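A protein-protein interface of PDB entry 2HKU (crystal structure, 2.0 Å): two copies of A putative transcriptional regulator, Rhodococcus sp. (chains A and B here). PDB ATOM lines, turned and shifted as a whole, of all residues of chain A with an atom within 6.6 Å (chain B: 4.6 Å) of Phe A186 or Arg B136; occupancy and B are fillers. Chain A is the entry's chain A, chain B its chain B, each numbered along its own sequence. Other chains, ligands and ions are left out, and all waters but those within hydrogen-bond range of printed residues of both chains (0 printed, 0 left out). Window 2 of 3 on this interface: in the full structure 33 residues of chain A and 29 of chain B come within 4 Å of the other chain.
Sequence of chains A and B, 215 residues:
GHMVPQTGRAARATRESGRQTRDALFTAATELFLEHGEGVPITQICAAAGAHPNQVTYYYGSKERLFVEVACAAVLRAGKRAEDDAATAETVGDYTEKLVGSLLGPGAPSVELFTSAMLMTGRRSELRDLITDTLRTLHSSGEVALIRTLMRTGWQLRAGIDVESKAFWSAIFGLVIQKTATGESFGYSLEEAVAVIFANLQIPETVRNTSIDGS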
ATOM      1  N   THR A 182     -24.892   9.288  24.721  1.00  0.00           N
ATOM      2  CA  THR A 182     -24.309  10.389  23.963  1.00  0.00           C
ATOM      3  C   THR A 182     -22.798  10.425  24.178  1.00  0.00           C
ATOM      4  O   THR A 182     -22.107  11.265  23.586  1.00  0.00           O
ATOM      5  CB  THR A 182     -24.831  11.734  24.446  1.00  0.00           C
ATOM      6  OG1 THR A 182     -24.680  11.804  25.857  1.00  0.00           O
ATOM      7  CG2 THR A 182     -26.310  11.913  24.054  1.00  0.00           C
ATOM      8  N   GLY A 183     -22.336   9.505  25.001  1.00  0.00           N
ATOM      9  CA  GLY A 183     -20.969   9.496  25.464  1.00  0.00           C
ATOM     10  C   GLY A 183     -20.645  10.792  26.208  1.00  0.00           C
ATOM     11  O   GLY A 183     -19.585  11.407  25.984  1.00  0.00           O
ATOM     12  N   GLU A 184     -21.551  11.231  27.076  1.00  0.00           N
ATOM     13  CA  GLU A 184     -21.328  12.452  27.845  1.00  0.00           C
ATOM     14  C   GLU A 184     -21.011  13.667  26.963  1.00  0.00           C
ATOM     15  O   GLU A 184     -20.021  14.417  27.176  1.00  0.00           O
ATOM     16  CB  GLU A 184     -20.206  12.249  28.895  1.00  0.00           C
ATOM     17  CG  GLU A 184     -20.548  11.277  29.972  1.00  0.00           C
ATOM     18  CD  GLU A 184     -19.410  10.328  30.287  1.00  0.00           C
ATOM     19  OE1 GLU A 184     -18.442  10.254  29.471  1.00  0.00           O
ATOM     20  OE2 GLU A 184     -19.512   9.637  31.345  1.00  0.00           O
ATOM     21  N   SER A 185     -21.883  13.919  26.003  1.00  0.00           N
ATOM     22  CA  SER A 185     -21.733  15.110  25.206  1.00  0.00           C
ATOM     23  C   SER A 185     -23.083  15.377  24.605  1.00  0.00           C
ATOM     24  O   SER A 185     -24.125  14.865  25.099  1.00  0.00           O
ATOM     25  CB  SER A 185     -20.601  14.970  24.167  1.00  0.00           C
ATOM     26  OG  SER A 185     -20.413  16.162  23.368  1.00  0.00           O
ATOM     27  N   PHE A 186     -23.086  16.229  23.584  1.00  0.00           N
ATOM     28  CA  PHE A 186     -24.310  16.687  22.951  1.00  0.00           C
ATOM     29  C   PHE A 186     -25.283  17.176  24.006  1.00  0.00           C
ATOM     30  O   PHE A 186     -26.487  16.880  23.963  1.00  0.00           O
ATOM     31  CB  PHE A 186     -24.894  15.570  22.045  1.00  0.00           C
ATOM     32  CG  PHE A 186     -23.883  15.037  21.044  1.00  0.00           C
ATOM     33  CD1 PHE A 186     -23.783  15.604  19.779  1.00  0.00           C
ATOM     34  CD2 PHE A 186     -22.990  14.011  21.392  1.00  0.00           C
ATOM     35  CE1 PHE A 186     -22.806  15.176  18.869  1.00  0.00           C
ATOM     36  CE2 PHE A 186     -22.038  13.557  20.479  1.00  0.00           C
ATOM     37  CZ  PHE A 186     -21.963  14.150  19.203  1.00  0.00           C
ATOM     38  N   GLY A 187     -24.772  17.986  24.931  1.00  0.00           N
ATOM     39  CA  GLY A 187     -25.638  18.588  25.981  1.00  0.00           C
ATOM     40  C   GLY A 187     -25.765  17.720  27.263  1.00  0.00           C
ATOM     41  O   GLY A 187     -26.344  18.154  28.233  1.00  0.00           O
ATOM     42  N   TYR A 188     -25.218  16.502  27.269  1.00  0.00           N
ATOM     43  CA  TYR A 188     -25.350  15.637  28.440  1.00  0.00           C
ATOM     44  C   TYR A 188     -23.997  15.233  28.967  1.00  0.00           C
ATOM     45  O   TYR A 188     -23.796  14.057  29.282  1.00  0.00           O
ATOM     46  CB  TYR A 188     -26.252  14.392  28.185  1.00  0.00           C
ATOM     47  CG  TYR A 188     -27.737  14.763  28.095  1.00  0.00           C
ATOM     48  CD1 TYR A 188     -28.473  15.015  29.233  1.00  0.00           C
ATOM     49  CD2 TYR A 188     -28.365  14.953  26.854  1.00  0.00           C
ATOM     50  CE1 TYR A 188     -29.872  15.433  29.178  1.00  0.00           C
ATOM     51  CE2 TYR A 188     -29.787  15.324  26.788  1.00  0.00           C
ATOM     52  CZ  TYR A 188     -30.521  15.552  27.966  1.00  0.00           C
ATOM     53  OH  TYR A 188     -31.904  15.904  27.899  1.00  0.00           O
ATOM     54  N   SER A 189     -23.042  16.179  29.014  1.00  0.00           N
ATOM     55  CA  SER A 189     -21.845  15.947  29.838  1.00  0.00           C
ATOM     56  C   SER A 189     -22.220  15.869  31.331  1.00  0.00           C
ATOM     57  O   SER A 189     -23.325  16.338  31.767  1.00  0.00           O
ATOM     58  CB  SER A 189     -20.796  17.086  29.631  1.00  0.00           C
ATOM     59  OG  SER A 189     -21.331  18.305  30.135  1.00  0.00           O
ATOM     60  N   GLU A 192     -23.307  19.311  32.564  1.00  0.00           N
ATOM     61  CA  GLU A 192     -24.576  19.696  32.054  1.00  0.00           C
ATOM     62  C   GLU A 192     -25.745  18.947  32.711  1.00  0.00           C
ATOM     63  O   GLU A 192     -26.735  19.579  32.983  1.00  0.00           O
ATOM     64  CB  GLU A 192     -24.618  19.508  30.559  1.00  0.00           C
ATOM     65  CG  GLU A 192     -23.782  20.608  29.875  1.00  0.00           C
ATOM     66  CD  GLU A 192     -23.564  20.263  28.421  1.00  0.00           C
ATOM     67  OE1 GLU A 192     -22.896  19.248  28.172  1.00  0.00           O
ATOM     68  OE2 GLU A 192     -24.166  20.945  27.566  1.00  0.00           O
ATOM     69  N   THR B 132     -27.716  10.371  18.605  1.00  0.00           N
ATOM     70  CA  THR B 132     -27.468  11.765  18.979  1.00  0.00           C
ATOM     71  C   THR B 132     -28.150  12.700  18.012  1.00  0.00           C
ATOM     72  O   THR B 132     -28.580  13.769  18.409  1.00  0.00           O
ATOM     73  CB  THR B 132     -25.921  12.091  19.156  1.00  0.00           C
ATOM     74  OG1 THR B 132     -25.250  12.019  17.915  1.00  0.00           O
ATOM     75  CG2 THR B 132     -25.306  11.051  20.036  1.00  0.00           C
ATOM     76  N   ASP B 133     -28.137  12.365  16.729  1.00  0.00           N
ATOM     77  CA  ASP B 133     -28.945  13.117  15.751  1.00  0.00           C
ATOM     78  C   ASP B 133     -30.433  13.195  16.125  1.00  0.00           C
ATOM     79  O   ASP B 133     -31.082  14.253  16.046  1.00  0.00           O
ATOM     80  CB  ASP B 133     -28.797  12.472  14.358  1.00  0.00           C
ATOM     81  CG  ASP B 133     -27.369  12.659  13.772  1.00  0.00           C
ATOM     82  OD1 ASP B 133     -26.532  13.488  14.344  1.00  0.00           O
ATOM     83  OD2 ASP B 133     -27.088  11.951  12.758  1.00  0.00           O
ATOM     84  N   THR B 134     -30.976  12.054  16.496  1.00  0.00           N
ATOM     85  CA  THR B 134     -32.385  11.948  16.947  1.00  0.00           C
ATOM     86  C   THR B 134     -32.631  12.756  18.227  1.00  0.00           C
ATOM     87  O   THR B 134     -33.579  13.466  18.323  1.00  0.00           O
ATOM     88  CB  THR B 134     -32.731  10.464  17.181  1.00  0.00           C
ATOM     89  OG1 THR B 134     -32.449   9.752  15.963  1.00  0.00           O
ATOM     90  CG2 THR B 134     -34.219  10.269  17.575  1.00  0.00           C
ATOM     91  N   LEU B 135     -31.753  12.661  19.239  1.00  0.00           N
ATOM     92  CA  LEU B 135     -31.931  13.446  20.422  1.00  0.00           C
ATOM     93  C   LEU B 135     -31.858  14.904  20.117  1.00  0.00           C
ATOM     94  O   LEU B 135     -32.542  15.623  20.739  1.00  0.00           O
ATOM     95  CB  LEU B 135     -30.821  13.167  21.548  1.00  0.00           C
ATOM     96  CG  LEU B 135     -30.936  11.837  22.321  1.00  0.00           C
ATOM     97  CD1 LEU B 135     -29.786  11.644  23.303  1.00  0.00           C
ATOM     98  CD2 LEU B 135     -32.266  11.694  23.103  1.00  0.00           C
ATOM     99  N   ARG B 136     -30.959  15.338  19.223  1.00  0.00           N
ATOM    100  CA  ARG B 136     -30.829  16.724  18.922  1.00  0.00           C
ATOM    101  C   ARG B 136     -32.158  17.190  18.290  1.00  0.00           C
ATOM    102  O   ARG B 136     -32.731  18.214  18.655  1.00  0.00           O
ATOM    103  CB  ARG B 136     -29.628  17.004  17.979  1.00  0.00           C
ATOM    104  CG  ARG B 136     -29.158  18.516  17.971  1.00  0.00           C
ATOM    105  CD  ARG B 136     -28.021  18.873  16.855  1.00  0.00           C
ATOM    106  NE  ARG B 136     -26.814  18.046  17.039  1.00  0.00           N
ATOM    107  CZ  ARG B 136     -26.550  16.948  16.344  1.00  0.00           C
ATOM    108  NH1 ARG B 136     -27.391  16.545  15.361  1.00  0.00           N
ATOM    109  NH2 ARG B 136     -25.445  16.267  16.630  1.00  0.00           N
ATOM    110  N   THR B 137     -32.691  16.394  17.410  1.00  0.00           N
ATOM    111  CA  THR B 137     -34.045  16.742  16.757  1.00  0.00           C
ATOM    112  C   THR B 137     -35.125  16.951  17.801  1.00  0.00           C
ATOM    113  O   THR B 137     -35.797  17.976  17.824  1.00  0.00           O
ATOM    114  CB  THR B 137     -34.438  15.661  15.743  1.00  0.00           C
ATOM    115  OG1 THR B 137     -33.490  15.673  14.689  1.00  0.00           O
ATOM    116  CG2 THR B 137     -35.900  15.892  15.091  1.00  0.00           C
ATOM    117  N   LEU B 138     -35.294  15.990  18.698  1.00  0.00           N
ATOM    118  CA  LEU B 138     -36.312  16.081  19.767  1.00  0.00           C
ATOM    119  C   LEU B 138     -36.134  17.352  20.608  1.00  0.00           C
ATOM    120  O   LEU B 138     -37.069  17.965  21.011  1.00  0.00           O
ATOM    121  CB  LEU B 138     -36.169  14.847  20.746  1.00  0.00           C
ATOM    122  CG  LEU B 138     -36.651  13.483  20.184  1.00  0.00           C
ATOM    123  CD1 LEU B 138     -36.367  12.253  21.086  1.00  0.00           C
ATOM    124  CD2 LEU B 138     -38.227  13.517  19.609  1.00  0.00           C
ATOM    125  N   HIS B 139     -34.904  17.582  21.058  1.00  0.00           N
ATOM    126  CA  HIS B 139     -34.608  18.701  21.907  1.00  0.00           C
ATOM    127  C   HIS B 139     -34.774  20.059  21.264  1.00  0.00           C
ATOM    128  O   HIS B 139     -35.181  21.009  21.935  1.00  0.00           O
ATOM    129  CB  HIS B 139     -33.153  18.582  22.468  1.00  0.00           C
ATOM    130  CG  HIS B 139     -33.046  17.620  23.591  1.00  0.00           C
ATOM    131  ND1 HIS B 139     -33.075  16.243  23.387  1.00  0.00           N
ATOM    132  CD2 HIS B 139     -32.871  17.800  24.933  1.00  0.00           C
ATOM    133  CE1 HIS B 139     -32.920  15.627  24.551  1.00  0.00           C
ATOM    134  NE2 HIS B 139     -32.789  16.542  25.498  1.00  0.00           N
ATOM    135  N   SER B 140     -34.342  20.174  20.000  1.00  0.00           N
ATOM    136  CA  SER B 140     -34.537  21.448  19.269  1.00  0.00           C
ATOM    137  C   SER B 140     -35.981  21.669  19.025  1.00  0.00           C
ATOM    138  O   SER B 140     -36.483  22.785  19.171  1.00  0.00           O
ATOM    139  CB  SER B 140     -33.745  21.454  17.948  1.00  0.00           C
ATOM    140  OG  SER B 140     -32.328  21.423  18.224  1.00  0.00           O
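The side-chain hydroxyl (OH) of Tyr A188 lies within hydrogen-bond range of a ring nitrogen (NE2) of His B139, at 2.6 Å.
The side-chain hydroxyl of Thr A182 lies close to the backbone NH of Glu A184 (3.4 Å).
The side-chain hydroxyl of Thr A182 is in hydrogen-bond range of the backbone carbonyl oxygen of Ser A185 (3.2 Å).
OD1 of Asp B133 is in salt-bridge range of NH1 of Arg B136, 3.3 Å away.
The backbone carbonyl oxygen (O) of Leu B135 lies within hydrogen-bond range of a ring nitrogen (ND1) of His B139 (2.8 Å).
The backbone carbonyl oxygen (O) of Arg B136 is in hydrogen-bond range of the side-chain hydroxyl (OG) of Ser B140 (3.3 Å).
Among the printed residues, pairs that only touch across the chains: Thr A182 with Leu B135 (3.6 Å), Phe A186 with Arg B136 (3.6 Å) and Phe A186 with Thr B132 (3.996 Å).
Printed residues of chain B within 4 Å of Phe A186: Thr B132 and Arg B136.
Arg B136 touches just one residue of chain A: Phe A186.
Of the printed residues of chain A, His B139 touches Tyr A188 (2.6 Å).
Of the printed residues of chain A, Thr B132 touches Phe A186 (3.996 Å).
Of the printed residues of chain B, Tyr A188 touches His B139 (2.6 Å).
The nearest printed residue of chain B that does not touch Phe A186 is Asp B133 (6.1 Å).
The nearest printed residue of chain A that does not touch Arg B136 is Thr A182 (7.5 Å).
Of the 9 printed residues of chain B, 4 touch a printed residue of chain A.
Hydrophobic or aromatic side chains of chain B within 4 Å of the printed part of chain A: Leu B135 and His B139.
Of the 9 printed residues of chain A, 3 touch a printed residue of chain B.
Hydrophobic or aromatic side chains of chain A within 4 Å of the printed part of chain B: Phe A186 and Tyr A188.
Among the printed residues, 4 pairs touch across the chains.
Among the printed residues, no Asp or Glu carboxylate lies within 4 Å of a Lys or Arg side-chain nitrogen of the other chain.
No position is printed for both chains.
Of the 4 pairs that touch across the chains among the printed residues, none has its exchanged pair printed and touching as well.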
